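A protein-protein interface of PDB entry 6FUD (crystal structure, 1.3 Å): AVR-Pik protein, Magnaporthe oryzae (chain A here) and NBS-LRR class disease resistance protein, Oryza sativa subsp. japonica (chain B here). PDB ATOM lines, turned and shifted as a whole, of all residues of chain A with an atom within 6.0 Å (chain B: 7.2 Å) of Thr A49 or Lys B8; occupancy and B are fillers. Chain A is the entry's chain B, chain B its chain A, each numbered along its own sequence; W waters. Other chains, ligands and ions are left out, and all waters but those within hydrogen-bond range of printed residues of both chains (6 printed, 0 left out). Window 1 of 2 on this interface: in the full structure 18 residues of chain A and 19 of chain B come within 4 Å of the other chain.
NZ of Lys B8 sits at hydrogen-bond distance from O of Thr A49, at 3.5 Å. The backbone carbonyl oxygen of Ala A47 is in hydrogen-bond range of the side-chain amide nitrogen of Gln B46 (3.0 Å). The side-chain carboxylate of Glu B74 sits close to the side-chain sulfur of Met A56 (3.8 Å).
The backbone carbonyl oxygen (O) of Met B6 sits at hydrogen-bond distance from the backbone NH (N) of Val B78, 2.9 Å away. The backbone NH (N) of Lys B8 lies within hydrogen-bond range of the backbone carbonyl oxygen (O) of Ser B76, at 2.8 Å. The backbone NH of Val B10 sits at hydrogen-bond distance from the backbone carbonyl oxygen of Glu B74 (2.9 Å). OE2 of Glu B74 lies within hydrogen-bond range of OG of Ser B76 (2.7 Å). O of Thr A49 is in hydrogen-bond range of NE1 of Trp A36 (3.4 Å).
Among the printed residues, merely in contact across the chains: Met A56 with Ser B76 and Tyr A51 with Val B78.
Of the printed residues of chain B, Ala A47 touches Gln B46. Printed residues of chain B within 4 Å of Thr A49: Lys B8 (3.5 Å). Lys B8 touches one residue of chain A. Of the printed residues of chain A, Glu B74 touches Met A56 (3.8 Å). Of the printed residues of chain A, Ser B76 touches Met A56. Printed residues of chain A within 4 Å of Val B78: Tyr A51 (3.7 Å). The nearest residue of chain B that does not touch Thr A49 is Glu B74 (4.9 Å). The nearest printed residue of chain A that does not touch Gln B46 is Trp A36 (4.1 Å).
Of the 17 printed residues of chain B, 5 touch a printed residue of chain A. Hydrophobic or aromatic side chains of chain B within 4 Å of the printed part of chain A: Val B78. Of the 15 printed residues of chain A, 4 touch a printed residue of chain B. Hydrophobic or aromatic side chains of chain A within 4 Å of the printed part of chain B: Tyr A51 and Met A56.
Water W3 lies within hydrogen-bond range of the side-chain carboxylate of Glu B74 (2.5 Å), the backbone carbonyl oxygen of Thr A49 (2.7 Å) and the indole nitrogen of Trp A36 (3.0 Å). Water W4 lies within hydrogen-bond range of OE2 of Glu B74, NZ of Lys B8 and O of Thr A49. Water W6 bridges OG1 of Thr A49 (2.7 Å) and NZ of Lys B8 (2.9 Å). Water W2 bridges NZ of Lys B8 (2.9 Å) and OH of Tyr A51 (3.1 Å). Water W5 bridges the side-chain amide oxygen (OE1) of Gln B46 (3.2 Å) and the backbone NH (N) of Thr A49 (3.3 Å). Water W1 bridges the backbone carbonyl oxygen (O) of Ala A47 (3.2 Å) and the side-chain amide oxygen (OE1) of Gln B46 (3.5 Å).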
ATOM      1  N   PRO A  21     -14.996 -20.946  12.179  1.00  0.00           N
ATOM      2  CA  PRO A  21     -16.134 -21.284  11.356  1.00  0.00           C
ATOM      3  C   PRO A  21     -16.899 -20.034  10.926  1.00  0.00           C
ATOM      4  O   PRO A  21     -16.836 -19.016  11.624  1.00  0.00           O
ATOM      5  CB  PRO A  21     -17.011 -22.166  12.261  1.00  0.00           C
ATOM      6  CG  PRO A  21     -16.025 -22.697  13.291  1.00  0.00           C
ATOM      7  CD  PRO A  21     -15.103 -21.507  13.532  1.00  0.00           C
ATOM      8  N   PHE A  23     -20.304 -18.743  10.907  1.00  0.00           N
ATOM      9  CA  PHE A  23     -21.502 -19.159  11.761  1.00  0.00           C
ATOM     10  C   PHE A  23     -22.390 -17.973  11.833  1.00  0.00           C
ATOM     11  O   PHE A  23     -22.002 -16.786  11.675  1.00  0.00           O
ATOM     12  CB  PHE A  23     -21.085 -19.578  13.150  1.00  0.00           C
ATOM     13  CG  PHE A  23     -20.423 -18.514  13.936  1.00  0.00           C
ATOM     14  CD1 PHE A  23     -19.039 -18.391  13.874  1.00  0.00           C
ATOM     15  CD2 PHE A  23     -21.149 -17.716  14.832  1.00  0.00           C
ATOM     16  CE1 PHE A  23     -18.387 -17.407  14.599  1.00  0.00           C
ATOM     17  CE2 PHE A  23     -20.492 -16.727  15.551  1.00  0.00           C
ATOM     18  CZ  PHE A  23     -19.111 -16.581  15.442  1.00  0.00           C
ATOM     19  N   PHE A  24     -23.620 -18.301  12.205  1.00  0.00           N
ATOM     20  CA  PHE A  24     -24.656 -17.328  12.434  1.00  0.00           C
ATOM     21  C   PHE A  24     -25.262 -17.679  13.783  1.00  0.00           C
ATOM     22  O   PHE A  24     -25.810 -18.789  13.874  1.00  0.00           O
ATOM     23  CB  PHE A  24     -25.682 -17.461  11.299  1.00  0.00           C
ATOM     24  CG  PHE A  24     -27.028 -16.835  11.594  1.00  0.00           C
ATOM     25  CD1 PHE A  24     -27.208 -15.474  11.476  1.00  0.00           C
ATOM     26  CD2 PHE A  24     -28.116 -17.625  12.002  1.00  0.00           C
ATOM     27  CE1 PHE A  24     -28.447 -14.893  11.762  1.00  0.00           C
ATOM     28  CE2 PHE A  24     -29.368 -17.054  12.279  1.00  0.00           C
ATOM     29  CZ  PHE A  24     -29.525 -15.683  12.163  1.00  0.00           C
ATOM     30  N   ASP A  25     -25.115 -16.837  14.834  1.00  0.00           N
ATOM     31  CA  ASP A  25     -25.762 -17.164  16.144  1.00  0.00           C
ATOM     32  C   ASP A  25     -27.219 -16.683  16.081  1.00  0.00           C
ATOM     33  O   ASP A  25     -27.536 -15.504  15.902  1.00  0.00           O
ATOM     34  CB  ASP A  25     -25.060 -16.540  17.339  1.00  0.00           C
ATOM     35  CG  ASP A  25     -23.738 -17.158  17.646  1.00  0.00           C
ATOM     36  OD1 ASP A  25     -23.597 -18.384  17.475  1.00  0.00           O
ATOM     37  OD2 ASP A  25     -22.848 -16.413  18.142  1.00  0.00           O
ATOM     38  N   PRO A  32     -24.668 -21.747  20.900  1.00  0.00           N
ATOM     39  CA  PRO A  32     -23.822 -22.937  21.045  1.00  0.00           C
ATOM     40  C   PRO A  32     -22.424 -22.593  21.476  1.00  0.00           C
ATOM     41  O   PRO A  32     -21.841 -21.645  20.992  1.00  0.00           O
ATOM     42  CB  PRO A  32     -23.871 -23.604  19.691  1.00  0.00           C
ATOM     43  CG  PRO A  32     -24.318 -22.565  18.742  1.00  0.00           C
ATOM     44  CD  PRO A  32     -25.143 -21.550  19.510  1.00  0.00           C
ATOM     45  N   CYS A  34     -19.548 -24.360  21.352  1.00  0.00           N
ATOM     46  CA  CYS A  34     -18.412 -25.012  20.723  1.00  0.00           C
ATOM     47  C   CYS A  34     -18.328 -24.672  19.214  1.00  0.00           C
ATOM     48  O   CYS A  34     -19.327 -24.498  18.552  1.00  0.00           O
ATOM     49  CB  CYS A  34     -18.524 -26.531  20.770  1.00  0.00           C
ATOM     50  SG  CYS A  34     -18.903 -27.224  22.389  1.00  0.00           S
ATOM     51  N   PHE A  35     -17.078 -24.636  18.755  1.00  0.00           N
ATOM     52  CA  PHE A  35     -16.774 -24.742  17.338  1.00  0.00           C
ATOM     53  C   PHE A  35     -16.444 -26.197  17.057  1.00  0.00           C
ATOM     54  O   PHE A  35     -15.776 -26.874  17.837  1.00  0.00           O
ATOM     55  CB  PHE A  35     -15.556 -23.887  16.929  1.00  0.00           C
ATOM     56  CG  PHE A  35     -15.740 -22.401  17.011  1.00  0.00           C
ATOM     57  CD1 PHE A  35     -16.924 -21.826  16.656  1.00  0.00           C
ATOM     58  CD2 PHE A  35     -14.690 -21.558  17.317  1.00  0.00           C
ATOM     59  CE1 PHE A  35     -17.077 -20.449  16.595  1.00  0.00           C
ATOM     60  CE2 PHE A  35     -14.845 -20.165  17.296  1.00  0.00           C
ATOM     61  CZ  PHE A  35     -16.024 -19.639  16.938  1.00  0.00           C
ATOM     62  N   TRP A  36     -16.868 -26.702  15.884  1.00  0.00           N
ATOM     63  CA  TRP A  36     -16.408 -27.990  15.377  1.00  0.00           C
ATOM     64  C   TRP A  36     -15.751 -27.811  14.004  1.00  0.00           C
ATOM     65  O   TRP A  36     -16.138 -26.911  13.241  1.00  0.00           O
ATOM     66  CB  TRP A  36     -17.544 -29.037  15.238  1.00  0.00           C
ATOM     67  CG  TRP A  36     -18.691 -28.695  14.337  1.00  0.00           C
ATOM     68  CD1 TRP A  36     -19.901 -28.190  14.710  1.00  0.00           C
ATOM     69  CD2 TRP A  36     -18.777 -28.889  12.915  1.00  0.00           C
ATOM     70  NE1 TRP A  36     -20.705 -28.016  13.625  1.00  0.00           N
ATOM     71  CE2 TRP A  36     -20.025 -28.433  12.505  1.00  0.00           C
ATOM     72  CE3 TRP A  36     -17.902 -29.367  11.955  1.00  0.00           C
ATOM     73  CZ2 TRP A  36     -20.421 -28.459  11.162  1.00  0.00           C
ATOM     74  CZ3 TRP A  36     -18.294 -29.370  10.625  1.00  0.00           C
ATOM     75  CH2 TRP A  36     -19.505 -28.912  10.246  1.00  0.00           C
ATOM     76  N   ALA A  47     -16.791 -26.556   8.846  1.00  0.00           N
ATOM     77  CA  ALA A  47     -16.738 -26.197  10.270  1.00  0.00           C
ATOM     78  C   ALA A  47     -18.047 -25.559  10.637  1.00  0.00           C
ATOM     79  O   ALA A  47     -18.751 -25.024   9.791  1.00  0.00           O
ATOM     80  CB  ALA A  47     -15.565 -25.267  10.514  1.00  0.00           C
ATOM     81  N   GLY A  48     -18.362 -25.568  11.938  1.00  0.00           N
ATOM     82  CA  GLY A  48     -19.601 -25.000  12.387  1.00  0.00           C
ATOM     83  C   GLY A  48     -19.617 -24.803  13.893  1.00  0.00           C
ATOM     84  O   GLY A  48     -18.569 -24.784  14.525  1.00  0.00           O
ATOM     85  N   THR A  49     -20.815 -24.712  14.460  1.00  0.00           N
ATOM     86  CA  THR A  49     -20.997 -24.557  15.909  1.00  0.00           C
ATOM     87  C   THR A  49     -21.863 -25.700  16.398  1.00  0.00           C
ATOM     88  O   THR A  49     -22.726 -26.210  15.685  1.00  0.00           O
ATOM     89  CB  THR A  49     -21.618 -23.213  16.275  1.00  0.00           C
ATOM     90  OG1 THR A  49     -22.907 -23.105  15.722  1.00  0.00           O
ATOM     91  CG2 THR A  49     -20.704 -22.054  15.896  1.00  0.00           C
ATOM     92  N   CYS A  50     -21.666 -26.068  17.682  1.00  0.00           N
ATOM     93  CA  CYS A  50     -22.513 -27.077  18.318  1.00  0.00           C
ATOM     94  C   CYS A  50     -22.510 -26.819  19.837  1.00  0.00           C
ATOM     95  O   CYS A  50     -21.654 -26.127  20.373  1.00  0.00           O
ATOM     96  CB  CYS A  50     -22.051 -28.504  17.994  1.00  0.00           C
ATOM     97  SG  CYS A  50     -20.404 -28.944  18.535  1.00  0.00           S
ATOM     98  N   TYR A  51     -23.460 -27.477  20.504  1.00  0.00           N
ATOM     99  CA  TYR A  51     -23.565 -27.350  21.974  1.00  0.00           C
ATOM    100  C   TYR A  51     -22.577 -28.229  22.690  1.00  0.00           C
ATOM    101  O   TYR A  51     -22.299 -29.351  22.277  1.00  0.00           O
ATOM    102  CB  TYR A  51     -25.005 -27.653  22.404  1.00  0.00           C
ATOM    103  CG  TYR A  51     -25.996 -26.622  21.916  1.00  0.00           C
ATOM    104  CD1 TYR A  51     -26.045 -25.363  22.472  1.00  0.00           C
ATOM    105  CD2 TYR A  51     -26.827 -26.884  20.877  1.00  0.00           C
ATOM    106  CE1 TYR A  51     -26.921 -24.399  22.033  1.00  0.00           C
ATOM    107  CE2 TYR A  51     -27.733 -25.935  20.378  1.00  0.00           C
ATOM    108  CZ  TYR A  51     -27.747 -24.689  20.941  1.00  0.00           C
ATOM    109  OH  TYR A  51     -28.621 -23.759  20.369  1.00  0.00           O
ATOM    110  N   MET A  56     -25.175 -34.972  18.840  1.00  0.00           N
ATOM    111  CA  MET A  56     -25.699 -34.707  17.523  1.00  0.00           C
ATOM    112  C   MET A  56     -25.390 -35.887  16.622  1.00  0.00           C
ATOM    113  O   MET A  56     -24.398 -36.572  16.839  1.00  0.00           O
ATOM    114  CB  MET A  56     -25.124 -33.406  16.928  1.00  0.00           C
ATOM    115  CG  MET A  56     -23.617 -33.403  16.810  1.00  0.00           C
ATOM    116  SD  MET A  56     -23.048 -31.749  16.179  1.00  0.00           S
ATOM    117  CE  MET A  56     -21.297 -31.985  16.281  1.00  0.00           C
ATOM    118  N   ARG A  90     -15.621 -22.053  22.324  1.00  0.00           N
ATOM    119  CA  ARG A  90     -15.603 -20.722  21.781  1.00  0.00           C
ATOM    120  C   ARG A  90     -15.038 -19.737  22.750  1.00  0.00           C
ATOM    121  O   ARG A  90     -15.265 -19.850  23.941  1.00  0.00           O
ATOM    122  CB  ARG A  90     -16.991 -20.282  21.337  1.00  0.00           C
ATOM    123  CG  ARG A  90     -17.500 -21.036  20.135  1.00  0.00           C
ATOM    124  CD  ARG A  90     -18.923 -20.702  19.815  1.00  0.00           C
ATOM    125  NE  ARG A  90     -19.159 -19.324  19.462  1.00  0.00           N
ATOM    126  CZ  ARG A  90     -20.322 -18.816  19.081  1.00  0.00           C
ATOM    127  NH1 ARG A  90     -21.369 -19.599  18.901  1.00  0.00           N
ATOM    128  NH2 ARG A  90     -20.412 -17.516  18.751  1.00  0.00           N
ATOM    129  N   GLU B   5     -38.403 -32.430  21.098  1.00  0.00           N
ATOM    130  CA  GLU B   5     -38.377 -30.938  21.291  1.00  0.00           C
ATOM    131  C   GLU B   5     -37.866 -30.218  20.042  1.00  0.00           C
ATOM    132  O   GLU B   5     -38.230 -30.606  18.945  1.00  0.00           O
ATOM    133  CB  GLU B   5     -37.593 -30.558  22.539  1.00  0.00           C
ATOM    134  CG  GLU B   5     -38.179 -31.166  23.797  1.00  0.00           C
ATOM    135  CD  GLU B   5     -38.124 -30.239  24.999  1.00  0.00           C
ATOM    136  OE1 GLU B   5     -37.083 -29.572  25.169  1.00  0.00           O
ATOM    137  OE2 GLU B   5     -39.112 -30.201  25.777  1.00  0.00           O
ATOM    138  N   MET B   6     -36.982 -29.233  20.174  1.00  0.00           N
ATOM    139  CA  MET B   6     -36.775 -28.314  19.064  1.00  0.00           C
ATOM    140  C   MET B   6     -35.685 -28.832  18.166  1.00  0.00           C
ATOM    141  O   MET B   6     -34.631 -29.198  18.643  1.00  0.00           O
ATOM    142  CB  MET B   6     -36.385 -26.992  19.612  1.00  0.00           C
ATOM    143  CG  MET B   6     -36.213 -25.901  18.593  1.00  0.00           C
ATOM    144  SD  MET B   6     -35.624 -24.372  19.326  1.00  0.00           S
ATOM    145  CE  MET B   6     -37.060 -23.921  20.220  1.00  0.00           C
ATOM    146  N   GLN B   7     -35.977 -28.892  16.875  1.00  0.00           N
ATOM    147  CA  GLN B   7     -35.092 -29.478  15.874  1.00  0.00           C
ATOM    148  C   GLN B   7     -34.032 -28.504  15.376  1.00  0.00           C
ATOM    149  O   GLN B   7     -34.324 -27.333  15.121  1.00  0.00           O
ATOM    150  CB  GLN B   7     -35.897 -29.897  14.642  1.00  0.00           C
ATOM    151  CG  GLN B   7     -36.915 -31.004  14.847  1.00  0.00           C
ATOM    152  CD  GLN B   7     -37.929 -31.033  13.727  1.00  0.00           C
ATOM    153  OE1 GLN B   7     -38.815 -30.170  13.647  1.00  0.00           O
ATOM    154  NE2 GLN B   7     -37.851 -32.056  12.884  1.00  0.00           N
ATOM    155  N   LYS B   8     -32.831 -29.021  15.192  1.00  0.00           N
ATOM    156  CA  LYS B   8     -31.812 -28.368  14.365  1.00  0.00           C
ATOM    157  C   LYS B   8     -31.427 -29.332  13.246  1.00  0.00           C
ATOM    158  O   LYS B   8     -31.036 -30.499  13.500  1.00  0.00           O
ATOM    159  CB  LYS B   8     -30.598 -28.087  15.221  1.00  0.00           C
ATOM    160  CG  LYS B   8     -29.513 -27.362  14.465  1.00  0.00           C
ATOM    161  CD  LYS B   8     -28.321 -27.088  15.382  1.00  0.00           C
ATOM    162  CE  LYS B   8     -27.252 -26.248  14.710  1.00  0.00           C
ATOM    163  NZ  LYS B   8     -26.207 -25.906  15.703  1.00  0.00           N
ATOM    164  N   ILE B   9     -31.545 -28.863  12.012  1.00  0.00           N
ATOM    165  CA  ILE B   9     -31.262 -29.689  10.858  1.00  0.00           C
ATOM    166  C   ILE B   9     -30.303 -28.864   9.996  1.00  0.00           C
ATOM    167  O   ILE B   9     -30.586 -27.702   9.684  1.00  0.00           O
ATOM    168  CB  ILE B   9     -32.532 -29.996  10.045  1.00  0.00           C
ATOM    169  CG1 ILE B   9     -33.528 -30.860  10.869  1.00  0.00           C
ATOM    170  CG2 ILE B   9     -32.161 -30.695   8.738  1.00  0.00           C
ATOM    171  CD1 ILE B   9     -34.993 -30.629  10.495  1.00  0.00           C
ATOM    172  N   VAL B  10     -29.173 -29.434   9.606  1.00  0.00           N
ATOM    173  CA  VAL B  10     -28.258 -28.703   8.716  1.00  0.00           C
ATOM    174  C   VAL B  10     -28.088 -29.528   7.453  1.00  0.00           C
ATOM    175  O   VAL B  10     -27.781 -30.729   7.504  1.00  0.00           O
ATOM    176  CB  VAL B  10     -26.893 -28.503   9.373  1.00  0.00           C
ATOM    177  CG1 VAL B  10     -26.039 -27.617   8.465  1.00  0.00           C
ATOM    178  CG2 VAL B  10     -27.053 -27.883  10.767  1.00  0.00           C
ATOM    179  N   GLN B  46     -23.817 -24.421   3.738  1.00  0.00           N
ATOM    180  CA  GLN B  46     -24.522 -24.980   4.900  1.00  0.00           C
ATOM    181  C   GLN B  46     -25.845 -24.235   5.074  1.00  0.00           C
ATOM    182  O   GLN B  46     -25.824 -23.019   5.194  1.00  0.00           O
ATOM    183  CB  GLN B  46     -23.658 -24.792   6.136  1.00  0.00           C
ATOM    184  CG  GLN B  46     -22.989 -25.985   6.652  1.00  0.00           C
ATOM    185  CD  GLN B  46     -22.290 -25.741   7.994  1.00  0.00           C
ATOM    186  OE1 GLN B  46     -22.884 -25.468   9.030  1.00  0.00           O
ATOM    187  NE2 GLN B  46     -21.003 -25.882   7.969  1.00  0.00           N
ATOM    188  N   VAL B  48     -28.694 -23.975   7.714  1.00  0.00           N
ATOM    189  CA  VAL B  48     -28.973 -24.298   9.108  1.00  0.00           C
ATOM    190  C   VAL B  48     -30.456 -23.974   9.373  1.00  0.00           C
ATOM    191  O   VAL B  48     -30.855 -22.827   9.266  1.00  0.00           O
ATOM    192  CB  VAL B  48     -28.064 -23.503  10.050  1.00  0.00           C
ATOM    193  CG1 VAL B  48     -28.421 -23.860  11.514  1.00  0.00           C
ATOM    194  CG2 VAL B  48     -26.599 -23.740   9.686  1.00  0.00           C
ATOM    195  N   VAL B  49     -31.242 -24.998   9.707  1.00  0.00           N
ATOM    196  CA  VAL B  49     -32.689 -24.885   9.906  1.00  0.00           C
ATOM    197  C   VAL B  49     -33.023 -25.208  11.363  1.00  0.00           C
ATOM    198  O   VAL B  49     -32.571 -26.212  11.871  1.00  0.00           O
ATOM    199  CB  VAL B  49     -33.455 -25.851   8.973  1.00  0.00           C
ATOM    200  CG1 VAL B  49     -34.946 -25.598   8.998  1.00  0.00           C
ATOM    201  CG2 VAL B  49     -32.903 -25.729   7.551  1.00  0.00           C
ATOM    202  N   VAL B  50     -33.812 -24.334  12.002  1.00  0.00           N
ATOM    203  CA  VAL B  50     -34.273 -24.595  13.359  1.00  0.00           C
ATOM    204  C   VAL B  50     -35.817 -24.498  13.344  1.00  0.00           C
ATOM    205  O   VAL B  50     -36.400 -23.614  12.671  1.00  0.00           O
ATOM    206  CB  VAL B  50     -33.682 -23.600  14.359  1.00  0.00           C
ATOM    207  CG1 VAL B  50     -34.338 -23.725  15.742  1.00  0.00           C
ATOM    208  CG2 VAL B  50     -32.192 -23.779  14.475  1.00  0.00           C
ATOM    209  N   GLY B  51     -36.471 -25.436  14.035  1.00  0.00           N
ATOM    210  CA  GLY B  51     -37.922 -25.375  14.194  1.00  0.00           C
ATOM    211  C   GLY B  51     -38.468 -26.486  15.029  1.00  0.00           C
ATOM    212  O   GLY B  51     -37.751 -27.024  15.865  1.00  0.00           O
ATOM    213  N   ILE B  54     -40.906 -30.052  11.852  1.00  0.00           N
ATOM    214  CA  ILE B  54     -40.434 -30.025  10.456  1.00  0.00           C
ATOM    215  C   ILE B  54     -40.351 -31.430   9.921  1.00  0.00           C
ATOM    216  O   ILE B  54     -39.750 -32.284  10.539  1.00  0.00           O
ATOM    217  CB  ILE B  54     -39.030 -29.373  10.322  1.00  0.00           C
ATOM    218  CG1 ILE B  54     -39.040 -27.969  10.912  1.00  0.00           C
ATOM    219  CG2 ILE B  54     -38.549 -29.391   8.851  1.00  0.00           C
ATOM    220  CD1 ILE B  54     -37.653 -27.446  11.170  1.00  0.00           C
ATOM    221  N   GLU B  74     -26.356 -32.630   9.436  1.00  0.00           N
ATOM    222  CA  GLU B  74     -26.610 -32.870  10.855  1.00  0.00           C
ATOM    223  C   GLU B  74     -28.079 -32.918  11.150  1.00  0.00           C
ATOM    224  O   GLU B  74     -28.854 -32.148  10.605  1.00  0.00           O
ATOM    225  CB  GLU B  74     -26.034 -31.708  11.612  1.00  0.00           C
ATOM    226  CG  GLU B  74     -26.346 -31.678  13.076  1.00  0.00           C
ATOM    227  CD  GLU B  74     -25.799 -30.463  13.760  1.00  0.00           C
ATOM    228  OE1 GLU B  74     -24.940 -29.762  13.181  1.00  0.00           O
ATOM    229  OE2 GLU B  74     -26.244 -30.162  14.907  1.00  0.00           O
ATOM    230  N   VAL B  75     -28.443 -33.791  12.103  1.00  0.00           N
ATOM    231  CA  VAL B  75     -29.762 -33.738  12.741  1.00  0.00           C
ATOM    232  C   VAL B  75     -29.519 -33.755  14.244  1.00  0.00           C
ATOM    233  O   VAL B  75     -28.818 -34.639  14.727  1.00  0.00           O
ATOM    234  CB  VAL B  75     -30.620 -34.930  12.323  1.00  0.00           C
ATOM    235  CG1 VAL B  75     -31.912 -34.909  13.067  1.00  0.00           C
ATOM    236  CG2 VAL B  75     -30.854 -34.897  10.817  1.00  0.00           C
ATOM    237  N   SER B  76     -30.051 -32.775  14.948  1.00  0.00           N
ATOM    238  CA  SER B  76     -29.874 -32.707  16.397  1.00  0.00           C
ATOM    239  C   SER B  76     -31.030 -31.956  17.036  1.00  0.00           C
ATOM    240  O   SER B  76     -31.909 -31.466  16.317  1.00  0.00           O
ATOM    241  CB  SER B  76     -28.499 -32.069  16.694  1.00  0.00           C
ATOM    242  OG  SER B  76     -28.477 -30.727  16.289  1.00  0.00           O
ATOM    243  N   GLN B  77     -31.008 -31.861  18.364  1.00  0.00           N
ATOM    244  CA  GLN B  77     -31.998 -31.077  19.117  1.00  0.00           C
ATOM    245  C   GLN B  77     -31.315 -29.850  19.685  1.00  0.00           C
ATOM    246  O   GLN B  77     -30.159 -29.924  20.072  1.00  0.00           O
ATOM    247  CB  GLN B  77     -32.633 -31.911  20.186  1.00  0.00           C
ATOM    248  CG  GLN B  77     -33.487 -33.030  19.558  1.00  0.00           C
ATOM    249  CD  GLN B  77     -34.915 -32.623  19.191  1.00  0.00           C
ATOM    250  OE1 GLN B  77     -35.358 -32.781  18.056  1.00  0.00           O
ATOM    251  NE2 GLN B  77     -35.641 -32.108  20.159  1.00  0.00           N
ATOM    252  N   VAL B  78     -32.024 -28.747  19.767  1.00  0.00           N
ATOM    253  CA  VAL B  78     -31.522 -27.566  20.421  1.00  0.00           C
ATOM    254  C   VAL B  78     -31.393 -27.832  21.925  1.00  0.00           C
ATOM    255  O   VAL B  78     -32.294 -28.413  22.533  1.00  0.00           O
ATOM    256  CB  VAL B  78     -32.415 -26.355  20.116  1.00  0.00           C
ATOM    257  CG1 VAL B  78     -31.985 -25.150  20.913  1.00  0.00           C
ATOM    258  CG2 VAL B  78     -32.431 -26.090  18.607  1.00  0.00           C
HETATM  259  O   HOH W   1     -21.052 -22.794  10.293  1.00  0.00           O
HETATM  260  O   HOH W   2     -27.618 -24.021  17.459  1.00  0.00           O
HETATM  261  O   HOH W   3     -23.650 -27.604  13.597  1.00  0.00           O
HETATM  262  O   HOH W   4     -25.028 -28.281  16.292  1.00  0.00           O
HETATM  263  O   HOH W   5     -23.042 -25.510  12.221  1.00  0.00           O
HETATM  264  O   HOH W   6     -24.705 -24.080  14.009  1.00  0.00           O
